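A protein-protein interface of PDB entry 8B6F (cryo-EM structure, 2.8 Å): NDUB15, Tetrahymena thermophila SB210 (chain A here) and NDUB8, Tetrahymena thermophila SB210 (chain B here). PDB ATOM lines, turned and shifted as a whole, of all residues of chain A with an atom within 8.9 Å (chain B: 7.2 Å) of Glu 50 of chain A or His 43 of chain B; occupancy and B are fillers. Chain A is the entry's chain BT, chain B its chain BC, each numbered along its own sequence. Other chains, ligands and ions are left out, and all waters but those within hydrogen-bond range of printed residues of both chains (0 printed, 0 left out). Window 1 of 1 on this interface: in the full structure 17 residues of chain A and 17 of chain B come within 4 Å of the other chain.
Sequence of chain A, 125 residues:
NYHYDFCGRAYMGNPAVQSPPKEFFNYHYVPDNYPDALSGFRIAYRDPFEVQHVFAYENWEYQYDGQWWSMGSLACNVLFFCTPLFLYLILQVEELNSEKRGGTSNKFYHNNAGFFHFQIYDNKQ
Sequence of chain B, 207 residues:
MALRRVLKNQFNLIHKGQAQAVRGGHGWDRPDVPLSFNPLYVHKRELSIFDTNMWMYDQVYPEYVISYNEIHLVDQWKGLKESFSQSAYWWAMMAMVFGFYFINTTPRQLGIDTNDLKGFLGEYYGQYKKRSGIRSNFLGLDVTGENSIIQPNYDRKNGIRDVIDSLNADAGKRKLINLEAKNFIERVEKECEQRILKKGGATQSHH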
ATOM      1  N   VAL A  17     -31.714 -17.129 -11.440  1.00  0.00           N
ATOM      2  CA  VAL A  17     -31.065 -16.969 -12.734  1.00  0.00           C
ATOM      3  C   VAL A  17     -31.255 -15.542 -13.229  1.00  0.00           C
ATOM      4  O   VAL A  17     -32.332 -14.947 -13.081  1.00  0.00           O
ATOM      5  CB  VAL A  17     -31.620 -17.993 -13.740  1.00  0.00           C
ATOM      6  CG1 VAL A  17     -31.313 -17.579 -15.176  1.00  0.00           C
ATOM      7  CG2 VAL A  17     -31.049 -19.368 -13.455  1.00  0.00           C
ATOM      8  N   GLN A  18     -30.201 -14.983 -13.822  1.00  0.00           N
ATOM      9  CA  GLN A  18     -30.222 -13.631 -14.354  1.00  0.00           C
ATOM     10  C   GLN A  18     -29.684 -13.636 -15.778  1.00  0.00           C
ATOM     11  O   GLN A  18     -28.960 -14.546 -16.189  1.00  0.00           O
ATOM     12  CB  GLN A  18     -29.385 -12.662 -13.505  1.00  0.00           C
ATOM     13  CG  GLN A  18     -29.556 -12.816 -12.001  1.00  0.00           C
ATOM     14  CD  GLN A  18     -28.250 -13.140 -11.305  1.00  0.00           C
ATOM     15  OE1 GLN A  18     -28.147 -14.125 -10.577  1.00  0.00           O
ATOM     16  NE2 GLN A  18     -27.243 -12.302 -11.522  1.00  0.00           N
ATOM     17  N   SER A  19     -30.053 -12.603 -16.528  1.00  0.00           N
ATOM     18  CA  SER A  19     -29.562 -12.452 -17.886  1.00  0.00           C
ATOM     19  C   SER A  19     -28.094 -12.025 -17.875  1.00  0.00           C
ATOM     20  O   SER A  19     -27.630 -11.393 -16.922  1.00  0.00           O
ATOM     21  CB  SER A  19     -30.397 -11.426 -18.646  1.00  0.00           C
ATOM     22  OG  SER A  19     -30.348 -10.159 -18.014  1.00  0.00           O
ATOM     23  N   PRO A  20     -27.342 -12.353 -18.924  1.00  0.00           N
ATOM     24  CA  PRO A  20     -25.933 -11.977 -18.948  1.00  0.00           C
ATOM     25  C   PRO A  20     -25.783 -10.471 -18.948  1.00  0.00           C
ATOM     26  O   PRO A  20     -26.655  -9.740 -19.455  1.00  0.00           O
ATOM     27  CB  PRO A  20     -25.423 -12.599 -20.255  1.00  0.00           C
ATOM     28  CG  PRO A  20     -26.631 -12.789 -21.092  1.00  0.00           C
ATOM     29  CD  PRO A  20     -27.739 -13.089 -20.136  1.00  0.00           C
ATOM     30  N   PRO A  21     -24.689  -9.954 -18.386  1.00  0.00           N
ATOM     31  CA  PRO A  21     -24.517  -8.497 -18.324  1.00  0.00           C
ATOM     32  C   PRO A  21     -24.155  -7.919 -19.683  1.00  0.00           C
ATOM     33  O   PRO A  21     -23.297  -8.449 -20.394  1.00  0.00           O
ATOM     34  CB  PRO A  21     -23.376  -8.310 -17.314  1.00  0.00           C
ATOM     35  CG  PRO A  21     -22.906  -9.697 -16.938  1.00  0.00           C
ATOM     36  CD  PRO A  21     -23.485 -10.655 -17.917  1.00  0.00           C
ATOM     37  N   PHE A  24     -19.649  -4.576 -18.973  1.00  0.00           N
ATOM     38  CA  PHE A  24     -18.816  -4.972 -17.847  1.00  0.00           C
ATOM     39  C   PHE A  24     -17.377  -4.589 -18.156  1.00  0.00           C
ATOM     40  O   PHE A  24     -16.990  -4.458 -19.319  1.00  0.00           O
ATOM     41  CB  PHE A  24     -18.927  -6.476 -17.573  1.00  0.00           C
ATOM     42  CG  PHE A  24     -18.683  -7.329 -18.785  1.00  0.00           C
ATOM     43  CD1 PHE A  24     -19.710  -7.605 -19.671  1.00  0.00           C
ATOM     44  CD2 PHE A  24     -17.429  -7.855 -19.037  1.00  0.00           C
ATOM     45  CE1 PHE A  24     -19.490  -8.388 -20.787  1.00  0.00           C
ATOM     46  CE2 PHE A  24     -17.201  -8.638 -20.153  1.00  0.00           C
ATOM     47  CZ  PHE A  24     -18.233  -8.904 -21.028  1.00  0.00           C
ATOM     48  N   PHE A  25     -16.590  -4.406 -17.099  1.00  0.00           N
ATOM     49  CA  PHE A  25     -15.175  -4.114 -17.279  1.00  0.00           C
ATOM     50  C   PHE A  25     -14.485  -5.274 -17.984  1.00  0.00           C
ATOM     51  O   PHE A  25     -14.788  -6.444 -17.732  1.00  0.00           O
ATOM     52  CB  PHE A  25     -14.510  -3.842 -15.931  1.00  0.00           C
ATOM     53  CG  PHE A  25     -15.075  -2.656 -15.207  1.00  0.00           C
ATOM     54  CD1 PHE A  25     -14.701  -1.372 -15.560  1.00  0.00           C
ATOM     55  CD2 PHE A  25     -15.972  -2.825 -14.167  1.00  0.00           C
ATOM     56  CE1 PHE A  25     -15.216  -0.278 -14.895  1.00  0.00           C
ATOM     57  CE2 PHE A  25     -16.490  -1.735 -13.497  1.00  0.00           C
ATOM     58  CZ  PHE A  25     -16.111  -0.460 -13.862  1.00  0.00           C
ATOM     59  N   ASN A  26     -13.554  -4.944 -18.874  1.00  0.00           N
ATOM     60  CA  ASN A  26     -12.894  -5.923 -19.723  1.00  0.00           C
ATOM     61  C   ASN A  26     -11.391  -5.686 -19.720  1.00  0.00           C
ATOM     62  O   ASN A  26     -10.907  -4.628 -19.309  1.00  0.00           O
ATOM     63  CB  ASN A  26     -13.421  -5.859 -21.162  1.00  0.00           C
ATOM     64  CG  ASN A  26     -13.963  -7.187 -21.644  1.00  0.00           C
ATOM     65  OD1 ASN A  26     -15.149  -7.313 -21.940  1.00  0.00           O
ATOM     66  ND2 ASN A  26     -13.093  -8.185 -21.733  1.00  0.00           N
ATOM     67  N   TYR A  27     -10.654  -6.697 -20.172  1.00  0.00           N
ATOM     68  CA  TYR A  27      -9.220  -6.548 -20.358  1.00  0.00           C
ATOM     69  C   TYR A  27      -8.930  -5.446 -21.369  1.00  0.00           C
ATOM     70  O   TYR A  27      -9.563  -5.365 -22.424  1.00  0.00           O
ATOM     71  CB  TYR A  27      -8.602  -7.860 -20.841  1.00  0.00           C
ATOM     72  CG  TYR A  27      -8.620  -8.973 -19.822  1.00  0.00           C
ATOM     73  CD1 TYR A  27      -9.752  -9.752 -19.634  1.00  0.00           C
ATOM     74  CD2 TYR A  27      -7.494  -9.256 -19.062  1.00  0.00           C
ATOM     75  CE1 TYR A  27      -9.766 -10.776 -18.709  1.00  0.00           C
ATOM     76  CE2 TYR A  27      -7.498 -10.276 -18.135  1.00  0.00           C
ATOM     77  CZ  TYR A  27      -8.637 -11.033 -17.963  1.00  0.00           C
ATOM     78  OH  TYR A  27      -8.642 -12.052 -17.040  1.00  0.00           O
ATOM     79  N   ALA A  44      -9.574 -17.494 -27.125  1.00  0.00           N
ATOM     80  CA  ALA A  44     -10.985 -17.837 -27.049  1.00  0.00           C
ATOM     81  C   ALA A  44     -11.794 -16.643 -26.563  1.00  0.00           C
ATOM     82  O   ALA A  44     -11.282 -15.760 -25.870  1.00  0.00           O
ATOM     83  CB  ALA A  44     -11.207 -19.024 -26.111  1.00  0.00           C
ATOM     84  N   TYR A  45     -13.070 -16.626 -26.934  1.00  0.00           N
ATOM     85  CA  TYR A  45     -13.963 -15.566 -26.489  1.00  0.00           C
ATOM     86  C   TYR A  45     -14.266 -15.715 -25.003  1.00  0.00           C
ATOM     87  O   TYR A  45     -14.626 -16.800 -24.536  1.00  0.00           O
ATOM     88  CB  TYR A  45     -15.257 -15.592 -27.301  1.00  0.00           C
ATOM     89  CG  TYR A  45     -16.063 -14.320 -27.187  1.00  0.00           C
ATOM     90  CD1 TYR A  45     -15.659 -13.160 -27.835  1.00  0.00           C
ATOM     91  CD2 TYR A  45     -17.232 -14.282 -26.438  1.00  0.00           C
ATOM     92  CE1 TYR A  45     -16.394 -11.993 -27.735  1.00  0.00           C
ATOM     93  CE2 TYR A  45     -17.975 -13.120 -26.331  1.00  0.00           C
ATOM     94  CZ  TYR A  45     -17.549 -11.979 -26.983  1.00  0.00           C
ATOM     95  OH  TYR A  45     -18.285 -10.822 -26.882  1.00  0.00           O
ATOM     96  N   ARG A  46     -14.125 -14.621 -24.263  1.00  0.00           N
ATOM     97  CA  ARG A  46     -14.223 -14.659 -22.813  1.00  0.00           C
ATOM     98  C   ARG A  46     -15.685 -14.673 -22.380  1.00  0.00           C
ATOM     99  O   ARG A  46     -16.547 -14.056 -23.010  1.00  0.00           O
ATOM    100  CB  ARG A  46     -13.501 -13.462 -22.195  1.00  0.00           C
ATOM    101  CG  ARG A  46     -12.044 -13.347 -22.611  1.00  0.00           C
ATOM    102  CD  ARG A  46     -11.324 -12.265 -21.827  1.00  0.00           C
ATOM    103  NE  ARG A  46      -9.923 -12.157 -22.214  1.00  0.00           N
ATOM    104  CZ  ARG A  46      -8.960 -12.963 -21.789  1.00  0.00           C
ATOM    105  NH1 ARG A  46      -9.212 -13.967 -20.965  1.00  0.00           N
ATOM    106  NH2 ARG A  46      -7.713 -12.757 -22.201  1.00  0.00           N
ATOM    107  N   ASP A  47     -15.956 -15.387 -21.297  1.00  0.00           N
ATOM    108  CA  ASP A  47     -17.313 -15.445 -20.763  1.00  0.00           C
ATOM    109  C   ASP A  47     -17.646 -14.140 -20.047  1.00  0.00           C
ATOM    110  O   ASP A  47     -16.857 -13.680 -19.218  1.00  0.00           O
ATOM    111  CB  ASP A  47     -17.458 -16.619 -19.802  1.00  0.00           C
ATOM    112  CG  ASP A  47     -18.858 -16.740 -19.237  1.00  0.00           C
ATOM    113  OD1 ASP A  47     -19.768 -17.160 -19.980  1.00  0.00           O
ATOM    114  OD2 ASP A  47     -19.050 -16.412 -18.049  1.00  0.00           O
ATOM    115  N   PRO A  48     -18.803 -13.530 -20.320  1.00  0.00           N
ATOM    116  CA  PRO A  48     -19.109 -12.242 -19.675  1.00  0.00           C
ATOM    117  C   PRO A  48     -19.165 -12.313 -18.160  1.00  0.00           C
ATOM    118  O   PRO A  48     -18.650 -11.414 -17.485  1.00  0.00           O
ATOM    119  CB  PRO A  48     -20.468 -11.865 -20.281  1.00  0.00           C
ATOM    120  CG  PRO A  48     -21.064 -13.151 -20.713  1.00  0.00           C
ATOM    121  CD  PRO A  48     -19.918 -14.004 -21.157  1.00  0.00           C
ATOM    122  N   PHE A  49     -19.788 -13.351 -17.601  1.00  0.00           N
ATOM    123  CA  PHE A  49     -19.847 -13.470 -16.148  1.00  0.00           C
ATOM    124  C   PHE A  49     -18.453 -13.614 -15.553  1.00  0.00           C
ATOM    125  O   PHE A  49     -18.144 -13.008 -14.522  1.00  0.00           O
ATOM    126  CB  PHE A  49     -20.716 -14.663 -15.751  1.00  0.00           C
ATOM    127  CG  PHE A  49     -22.188 -14.409 -15.874  1.00  0.00           C
ATOM    128  CD1 PHE A  49     -22.811 -13.469 -15.073  1.00  0.00           C
ATOM    129  CD2 PHE A  49     -22.954 -15.134 -16.770  1.00  0.00           C
ATOM    130  CE1 PHE A  49     -24.168 -13.239 -15.177  1.00  0.00           C
ATOM    131  CE2 PHE A  49     -24.311 -14.911 -16.879  1.00  0.00           C
ATOM    132  CZ  PHE A  49     -24.919 -13.961 -16.082  1.00  0.00           C
ATOM    133  N   GLU A  50     -17.603 -14.426 -16.180  1.00  0.00           N
ATOM    134  CA  GLU A  50     -16.258 -14.631 -15.656  1.00  0.00           C
ATOM    135  C   GLU A  50     -15.441 -13.346 -15.703  1.00  0.00           C
ATOM    136  O   GLU A  50     -14.756 -13.008 -14.734  1.00  0.00           O
ATOM    137  CB  GLU A  50     -15.565 -15.747 -16.434  1.00  0.00           C
ATOM    138  CG  GLU A  50     -16.232 -17.101 -16.251  1.00  0.00           C
ATOM    139  CD  GLU A  50     -15.642 -18.171 -17.143  1.00  0.00           C
ATOM    140  OE1 GLU A  50     -14.880 -17.823 -18.069  1.00  0.00           O
ATOM    141  OE2 GLU A  50     -15.939 -19.361 -16.918  1.00  0.00           O
ATOM    142  N   VAL A  51     -15.533 -12.596 -16.801  1.00  0.00           N
ATOM    143  CA  VAL A  51     -14.804 -11.333 -16.893  1.00  0.00           C
ATOM    144  C   VAL A  51     -15.337 -10.339 -15.871  1.00  0.00           C
ATOM    145  O   VAL A  51     -14.571  -9.603 -15.239  1.00  0.00           O
ATOM    146  CB  VAL A  51     -14.872 -10.768 -18.323  1.00  0.00           C
ATOM    147  CG1 VAL A  51     -14.075  -9.479 -18.421  1.00  0.00           C
ATOM    148  CG2 VAL A  51     -14.337 -11.776 -19.318  1.00  0.00           C
ATOM    149  N   GLN A  52     -16.656 -10.294 -15.696  1.00  0.00           N
ATOM    150  CA  GLN A  52     -17.246  -9.399 -14.707  1.00  0.00           C
ATOM    151  C   GLN A  52     -16.728  -9.714 -13.310  1.00  0.00           C
ATOM    152  O   GLN A  52     -16.376  -8.806 -12.551  1.00  0.00           O
ATOM    153  CB  GLN A  52     -18.770  -9.508 -14.753  1.00  0.00           C
ATOM    154  CG  GLN A  52     -19.494  -8.503 -13.877  1.00  0.00           C
ATOM    155  CD  GLN A  52     -20.986  -8.753 -13.828  1.00  0.00           C
ATOM    156  OE1 GLN A  52     -21.439  -9.890 -13.953  1.00  0.00           O
ATOM    157  NE2 GLN A  52     -21.760  -7.690 -13.653  1.00  0.00           N
ATOM    158  N   HIS A  53     -16.669 -10.998 -12.955  1.00  0.00           N
ATOM    159  CA  HIS A  53     -16.106 -11.387 -11.666  1.00  0.00           C
ATOM    160  C   HIS A  53     -14.631 -11.018 -11.572  1.00  0.00           C
ATOM    161  O   HIS A  53     -14.159 -10.588 -10.514  1.00  0.00           O
ATOM    162  CB  HIS A  53     -16.289 -12.885 -11.434  1.00  0.00           C
ATOM    163  CG  HIS A  53     -15.677 -13.370 -10.156  1.00  0.00           C
ATOM    164  ND1 HIS A  53     -14.331 -13.632 -10.025  1.00  0.00           N
ATOM    165  CD2 HIS A  53     -16.229 -13.635  -8.949  1.00  0.00           C
ATOM    166  CE1 HIS A  53     -14.081 -14.038  -8.794  1.00  0.00           C
ATOM    167  NE2 HIS A  53     -15.216 -14.048  -8.120  1.00  0.00           N
ATOM    168  N   VAL A  54     -13.883 -11.180 -12.664  1.00  0.00           N
ATOM    169  CA  VAL A  54     -12.458 -10.862 -12.636  1.00  0.00           C
ATOM    170  C   VAL A  54     -12.239  -9.406 -12.253  1.00  0.00           C
ATOM    171  O   VAL A  54     -11.352  -9.088 -11.453  1.00  0.00           O
ATOM    172  CB  VAL A  54     -11.821 -11.176 -14.005  1.00  0.00           C
ATOM    173  CG1 VAL A  54     -10.413 -10.613 -14.094  1.00  0.00           C
ATOM    174  CG2 VAL A  54     -11.763 -12.661 -14.238  1.00  0.00           C
ATOM    175  N   PHE A  55     -13.032  -8.500 -12.816  1.00  0.00           N
ATOM    176  CA  PHE A  55     -12.801  -7.072 -12.650  1.00  0.00           C
ATOM    177  C   PHE A  55     -13.738  -6.416 -11.643  1.00  0.00           C
ATOM    178  O   PHE A  55     -13.658  -5.199 -11.456  1.00  0.00           O
ATOM    179  CB  PHE A  55     -12.918  -6.374 -14.006  1.00  0.00           C
ATOM    180  CG  PHE A  55     -11.736  -6.606 -14.897  1.00  0.00           C
ATOM    181  CD1 PHE A  55     -10.601  -5.822 -14.780  1.00  0.00           C
ATOM    182  CD2 PHE A  55     -11.752  -7.621 -15.839  1.00  0.00           C
ATOM    183  CE1 PHE A  55      -9.509  -6.041 -15.591  1.00  0.00           C
ATOM    184  CE2 PHE A  55     -10.663  -7.843 -16.652  1.00  0.00           C
ATOM    185  CZ  PHE A  55      -9.541  -7.051 -16.530  1.00  0.00           C
ATOM    186  N   ALA A  56     -14.611  -7.178 -10.984  1.00  0.00           N
ATOM    187  CA  ALA A  56     -15.552  -6.568 -10.049  1.00  0.00           C
ATOM    188  C   ALA A  56     -14.856  -6.082  -8.783  1.00  0.00           C
ATOM    189  O   ALA A  56     -15.077  -4.949  -8.340  1.00  0.00           O
ATOM    190  CB  ALA A  56     -16.658  -7.563  -9.698  1.00  0.00           C
ATOM    191  N   TYR B  41     -20.448 -26.659 -18.350  1.00  0.00           N
ATOM    192  CA  TYR B  41     -21.259 -25.861 -17.440  1.00  0.00           C
ATOM    193  C   TYR B  41     -21.306 -24.419 -17.933  1.00  0.00           C
ATOM    194  O   TYR B  41     -20.258 -23.790 -18.108  1.00  0.00           O
ATOM    195  CB  TYR B  41     -20.702 -25.935 -16.020  1.00  0.00           C
ATOM    196  CG  TYR B  41     -21.429 -25.051 -15.037  1.00  0.00           C
ATOM    197  CD1 TYR B  41     -22.581 -25.492 -14.403  1.00  0.00           C
ATOM    198  CD2 TYR B  41     -20.963 -23.781 -14.738  1.00  0.00           C
ATOM    199  CE1 TYR B  41     -23.250 -24.692 -13.505  1.00  0.00           C
ATOM    200  CE2 TYR B  41     -21.626 -22.972 -13.839  1.00  0.00           C
ATOM    201  CZ  TYR B  41     -22.769 -23.434 -13.226  1.00  0.00           C
ATOM    202  OH  TYR B  41     -23.435 -22.634 -12.329  1.00  0.00           O
ATOM    203  N   VAL B  42     -22.510 -23.900 -18.149  1.00  0.00           N
ATOM    204  CA  VAL B  42     -22.707 -22.541 -18.644  1.00  0.00           C
ATOM    205  C   VAL B  42     -23.174 -21.678 -17.481  1.00  0.00           C
ATOM    206  O   VAL B  42     -24.119 -22.039 -16.769  1.00  0.00           O
ATOM    207  CB  VAL B  42     -23.711 -22.499 -19.809  1.00  0.00           C
ATOM    208  CG1 VAL B  42     -23.214 -23.349 -20.964  1.00  0.00           C
ATOM    209  CG2 VAL B  42     -25.091 -22.966 -19.366  1.00  0.00           C
ATOM    210  N   HIS B  43     -22.500 -20.550 -17.277  1.00  0.00           N
ATOM    211  CA  HIS B  43     -22.844 -19.661 -16.177  1.00  0.00           C
ATOM    212  C   HIS B  43     -24.125 -18.900 -16.490  1.00  0.00           C
ATOM    213  O   HIS B  43     -24.273 -18.331 -17.575  1.00  0.00           O
ATOM    214  CB  HIS B  43     -21.702 -18.684 -15.906  1.00  0.00           C
ATOM    215  CG  HIS B  43     -20.452 -19.343 -15.413  1.00  0.00           C
ATOM    216  ND1 HIS B  43     -20.082 -19.334 -14.086  1.00  0.00           N
ATOM    217  CD2 HIS B  43     -19.491 -20.033 -16.067  1.00  0.00           C
ATOM    218  CE1 HIS B  43     -18.945 -19.990 -13.944  1.00  0.00           C
ATOM    219  NE2 HIS B  43     -18.565 -20.425 -15.131  1.00  0.00           N
ATOM    220  N   LYS B  44     -25.051 -18.895 -15.534  1.00  0.00           N
ATOM    221  CA  LYS B  44     -26.306 -18.170 -15.661  1.00  0.00           C
ATOM    222  C   LYS B  44     -26.522 -17.170 -14.537  1.00  0.00           C
ATOM    223  O   LYS B  44     -27.524 -16.448 -14.555  1.00  0.00           O
ATOM    224  CB  LYS B  44     -27.484 -19.151 -15.698  1.00  0.00           C
ATOM    225  CG  LYS B  44     -27.391 -20.175 -16.821  1.00  0.00           C
ATOM    226  CD  LYS B  44     -28.599 -21.102 -16.843  1.00  0.00           C
ATOM    227  CE  LYS B  44     -28.687 -21.963 -15.591  1.00  0.00           C
ATOM    228  NZ  LYS B  44     -27.442 -22.744 -15.347  1.00  0.00           N
ATOM    229  N   ARG B  45     -25.618 -17.108 -13.562  1.00  0.00           N
ATOM    230  CA  ARG B  45     -25.740 -16.208 -12.427  1.00  0.00           C
ATOM    231  C   ARG B  45     -24.418 -15.495 -12.204  1.00  0.00           C
ATOM    232  O   ARG B  45     -23.345 -16.041 -12.475  1.00  0.00           O
ATOM    233  CB  ARG B  45     -26.141 -16.964 -11.155  1.00  0.00           C
ATOM    234  CG  ARG B  45     -27.403 -17.786 -11.315  1.00  0.00           C
ATOM    235  CD  ARG B  45     -27.583 -18.763 -10.175  1.00  0.00           C
ATOM    236  NE  ARG B  45     -28.677 -19.685 -10.445  1.00  0.00           N
ATOM    237  CZ  ARG B  45     -28.588 -20.741 -11.243  1.00  0.00           C
ATOM    238  NH1 ARG B  45     -27.462 -21.043 -11.866  1.00  0.00           N
ATOM    239  NH2 ARG B  45     -29.657 -21.509 -11.421  1.00  0.00           N
ATOM    240  N   GLU B  46     -24.504 -14.267 -11.705  1.00  0.00           N
ATOM    241  CA  GLU B  46     -23.303 -13.496 -11.429  1.00  0.00           C
ATOM    242  C   GLU B  46     -22.510 -14.143 -10.303  1.00  0.00           C
ATOM    243  O   GLU B  46     -23.070 -14.571  -9.291  1.00  0.00           O
ATOM    244  CB  GLU B  46     -23.667 -12.060 -11.055  1.00  0.00           C
ATOM    245  CG  GLU B  46     -22.478 -11.231 -10.592  1.00  0.00           C
ATOM    246  CD  GLU B  46     -22.815  -9.764 -10.435  1.00  0.00           C
ATOM    247  OE1 GLU B  46     -23.877  -9.339 -10.936  1.00  0.00           O
ATOM    248  OE2 GLU B  46     -22.017  -9.033  -9.810  1.00  0.00           O
ATOM    249  N   LEU B  47     -21.196 -14.214 -10.489  1.00  0.00           N
ATOM    250  CA  LEU B  47     -20.294 -14.726  -9.461  1.00  0.00           C
ATOM    251  C   LEU B  47     -19.999 -13.579  -8.506  1.00  0.00           C
ATOM    252  O   LEU B  47     -19.118 -12.755  -8.756  1.00  0.00           O
ATOM    253  CB  LEU B  47     -19.019 -15.285 -10.082  1.00  0.00           C
ATOM    254  CG  LEU B  47     -19.147 -16.477 -11.041  1.00  0.00           C
ATOM    255  CD1 LEU B  47     -19.697 -16.069 -12.401  1.00  0.00           C
ATOM    256  CD2 LEU B  47     -17.814 -17.183 -11.206  1.00  0.00           C
ATOM    257  N   TYR B  57     -14.773 -23.855  -7.886  1.00  0.00           N
ATOM    258  CA  TYR B  57     -15.025 -23.549  -9.286  1.00  0.00           C
ATOM    259  C   TYR B  57     -14.641 -24.721 -10.177  1.00  0.00           C
ATOM    260  O   TYR B  57     -13.612 -25.370  -9.975  1.00  0.00           O
ATOM    261  CB  TYR B  57     -14.246 -22.300  -9.700  1.00  0.00           C
ATOM    262  CG  TYR B  57     -14.601 -21.075  -8.890  1.00  0.00           C
ATOM    263  CD1 TYR B  57     -15.738 -20.336  -9.178  1.00  0.00           C
ATOM    264  CD2 TYR B  57     -13.796 -20.658  -7.842  1.00  0.00           C
ATOM    265  CE1 TYR B  57     -16.067 -19.217  -8.440  1.00  0.00           C
ATOM    266  CE2 TYR B  57     -14.115 -19.542  -7.098  1.00  0.00           C
ATOM    267  CZ  TYR B  57     -15.251 -18.825  -7.403  1.00  0.00           C
ATOM    268  OH  TYR B  57     -15.574 -17.710  -6.665  1.00  0.00           O
ATOM    269  N   ASP B  58     -15.486 -24.993 -11.168  1.00  0.00           N
ATOM    270  CA  ASP B  58     -15.219 -26.039 -12.142  1.00  0.00           C
ATOM    271  C   ASP B  58     -15.945 -25.693 -13.431  1.00  0.00           C
ATOM    272  O   ASP B  58     -16.902 -24.916 -13.437  1.00  0.00           O
ATOM    273  CB  ASP B  58     -15.659 -27.413 -11.628  1.00  0.00           C
ATOM    274  CG  ASP B  58     -15.169 -28.545 -12.505  1.00  0.00           C
ATOM    275  OD1 ASP B  58     -14.412 -28.271 -13.456  1.00  0.00           O
ATOM    276  OD2 ASP B  58     -15.539 -29.708 -12.243  1.00  0.00           O
ATOM    277  N   GLN B  59     -15.474 -26.276 -14.528  1.00  0.00           N
ATOM    278  CA  GLN B  59     -16.067 -26.051 -15.838  1.00  0.00           C
ATOM    279  C   GLN B  59     -17.092 -27.111 -16.216  1.00  0.00           C
ATOM    280  O   GLN B  59     -17.709 -26.999 -17.279  1.00  0.00           O
ATOM    281  CB  GLN B  59     -14.970 -25.994 -16.904  1.00  0.00           C
ATOM    282  CG  GLN B  59     -13.934 -24.914 -16.646  1.00  0.00           C
ATOM    283  CD  GLN B  59     -12.866 -24.868 -17.711  1.00  0.00           C
ATOM    284  OE1 GLN B  59     -12.963 -25.543 -18.734  1.00  0.00           O
ATOM    285  NE2 GLN B  59     -11.833 -24.069 -17.477  1.00  0.00           N
ATOM    286  N   PRO B  62     -19.319 -27.571 -11.081  1.00  0.00           N
ATOM    287  CA  PRO B  62     -18.976 -26.693  -9.958  1.00  0.00           C
ATOM    288  C   PRO B  62     -19.764 -27.069  -8.713  1.00  0.00           C
ATOM    289  O   PRO B  62     -20.908 -27.519  -8.788  1.00  0.00           O
ATOM    290  CB  PRO B  62     -19.355 -25.297 -10.468  1.00  0.00           C
ATOM    291  CG  PRO B  62     -20.357 -25.540 -11.532  1.00  0.00           C
ATOM    292  CD  PRO B  62     -19.982 -26.841 -12.172  1.00  0.00           C
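The backbone NH (N) of Gln 18 of chain A sits at hydrogen-bond distance from the backbone carbonyl oxygen (O) of Lys 44 of chain B (3.1 Å).
OE2 of Glu 50 of chain A is in hydrogen-bond range of NE2 of His 43 of chain B, at 3.3 Å.
N of Glu 46 of chain B sits close to NE2 of Gln 18 of chain A, 3.4 Å away.
N of Phe 49 of chain A is in hydrogen-bond range of OD2 of Asp 47 of chain A, at 3.2 Å.
The backbone NH (N) of Glu 50 of chain A is in hydrogen-bond range of the side-chain carboxylate (OD2) of Asp 47 of chain A.
Val 17 of chain A touches Arg 45 of chain B (CG2 to NH2, 3.3 Å).
Arg 45 of chain B touches Gln 18 of chain A (CB to OE1, 3.5 Å).
Phe 49 of chain A touches His 43 of chain B (CE2 to O, 3.5 Å).
CZ of Phe 49 of chain A touches C of Lys 44 of chain B, 3.9 Å away.
O of Arg 45 of chain B touches CD1 of Phe 49 of chain A, at 3.7 Å.
N of Glu 46 of chain B touches CE1 of Phe 49 of chain A, 3.6 Å away.
Phe 49 of chain A touches Leu 47 of chain B.
Gln 52 of chain A touches Glu 46 of chain B.
O of Leu 47 of chain B touches CD2 of His 53 of chain A (3.0 Å).
NE2 of His 53 of chain A touches OH of Tyr 57 of chain B (3.96 Å).
Glu 50 of chain A touches just one residue of chain B: His 43.
Of the printed residues of chain A, His 43 of chain B touches Phe 49 (3.5 Å) and Glu 50 (3.3 Å).
No residue of chain A comes within 4 Å of Val 42 of chain B.
Of the printed residues of chain A, Leu 47 of chain B touches Phe 49 and His 53.
Of the printed residues of chain B, Phe 49 of chain A touches His 43 (3.5 Å), Lys 44 (3.9 Å), Arg 45 (3.7 Å), Glu 46 (3.6 Å) and Leu 47 (3.8 Å).
Of the printed residues of chain B, Val 17 of chain A touches Arg 45 (3.3 Å).
Of the printed residues of chain B, Gln 52 of chain A touches Glu 46 (3.8 Å).
Of the printed residues of chain B, His 53 of chain A touches Leu 47 (3.0 Å) and Tyr 57 (3.96 Å).
Ala 56 of chain A touches none of the printed residues of chain B.
The nearest residue of chain B that does not touch Glu 50 of chain A is Leu 47 of chain B (4.6 Å).
Printed residues of chain B that touch a printed residue of chain A: His 43, Lys 44, Arg 45, Glu 46, Leu 47 and Tyr 57.
Hydrophobic or aromatic side chains of chain B within 4 Å of the printed part of chain A: His 43, Leu 47 and Tyr 57.
Of the 22 printed residues of chain A, 6 touch a printed residue of chain B.
Among the printed residues, 13 pairs touch across the chains.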
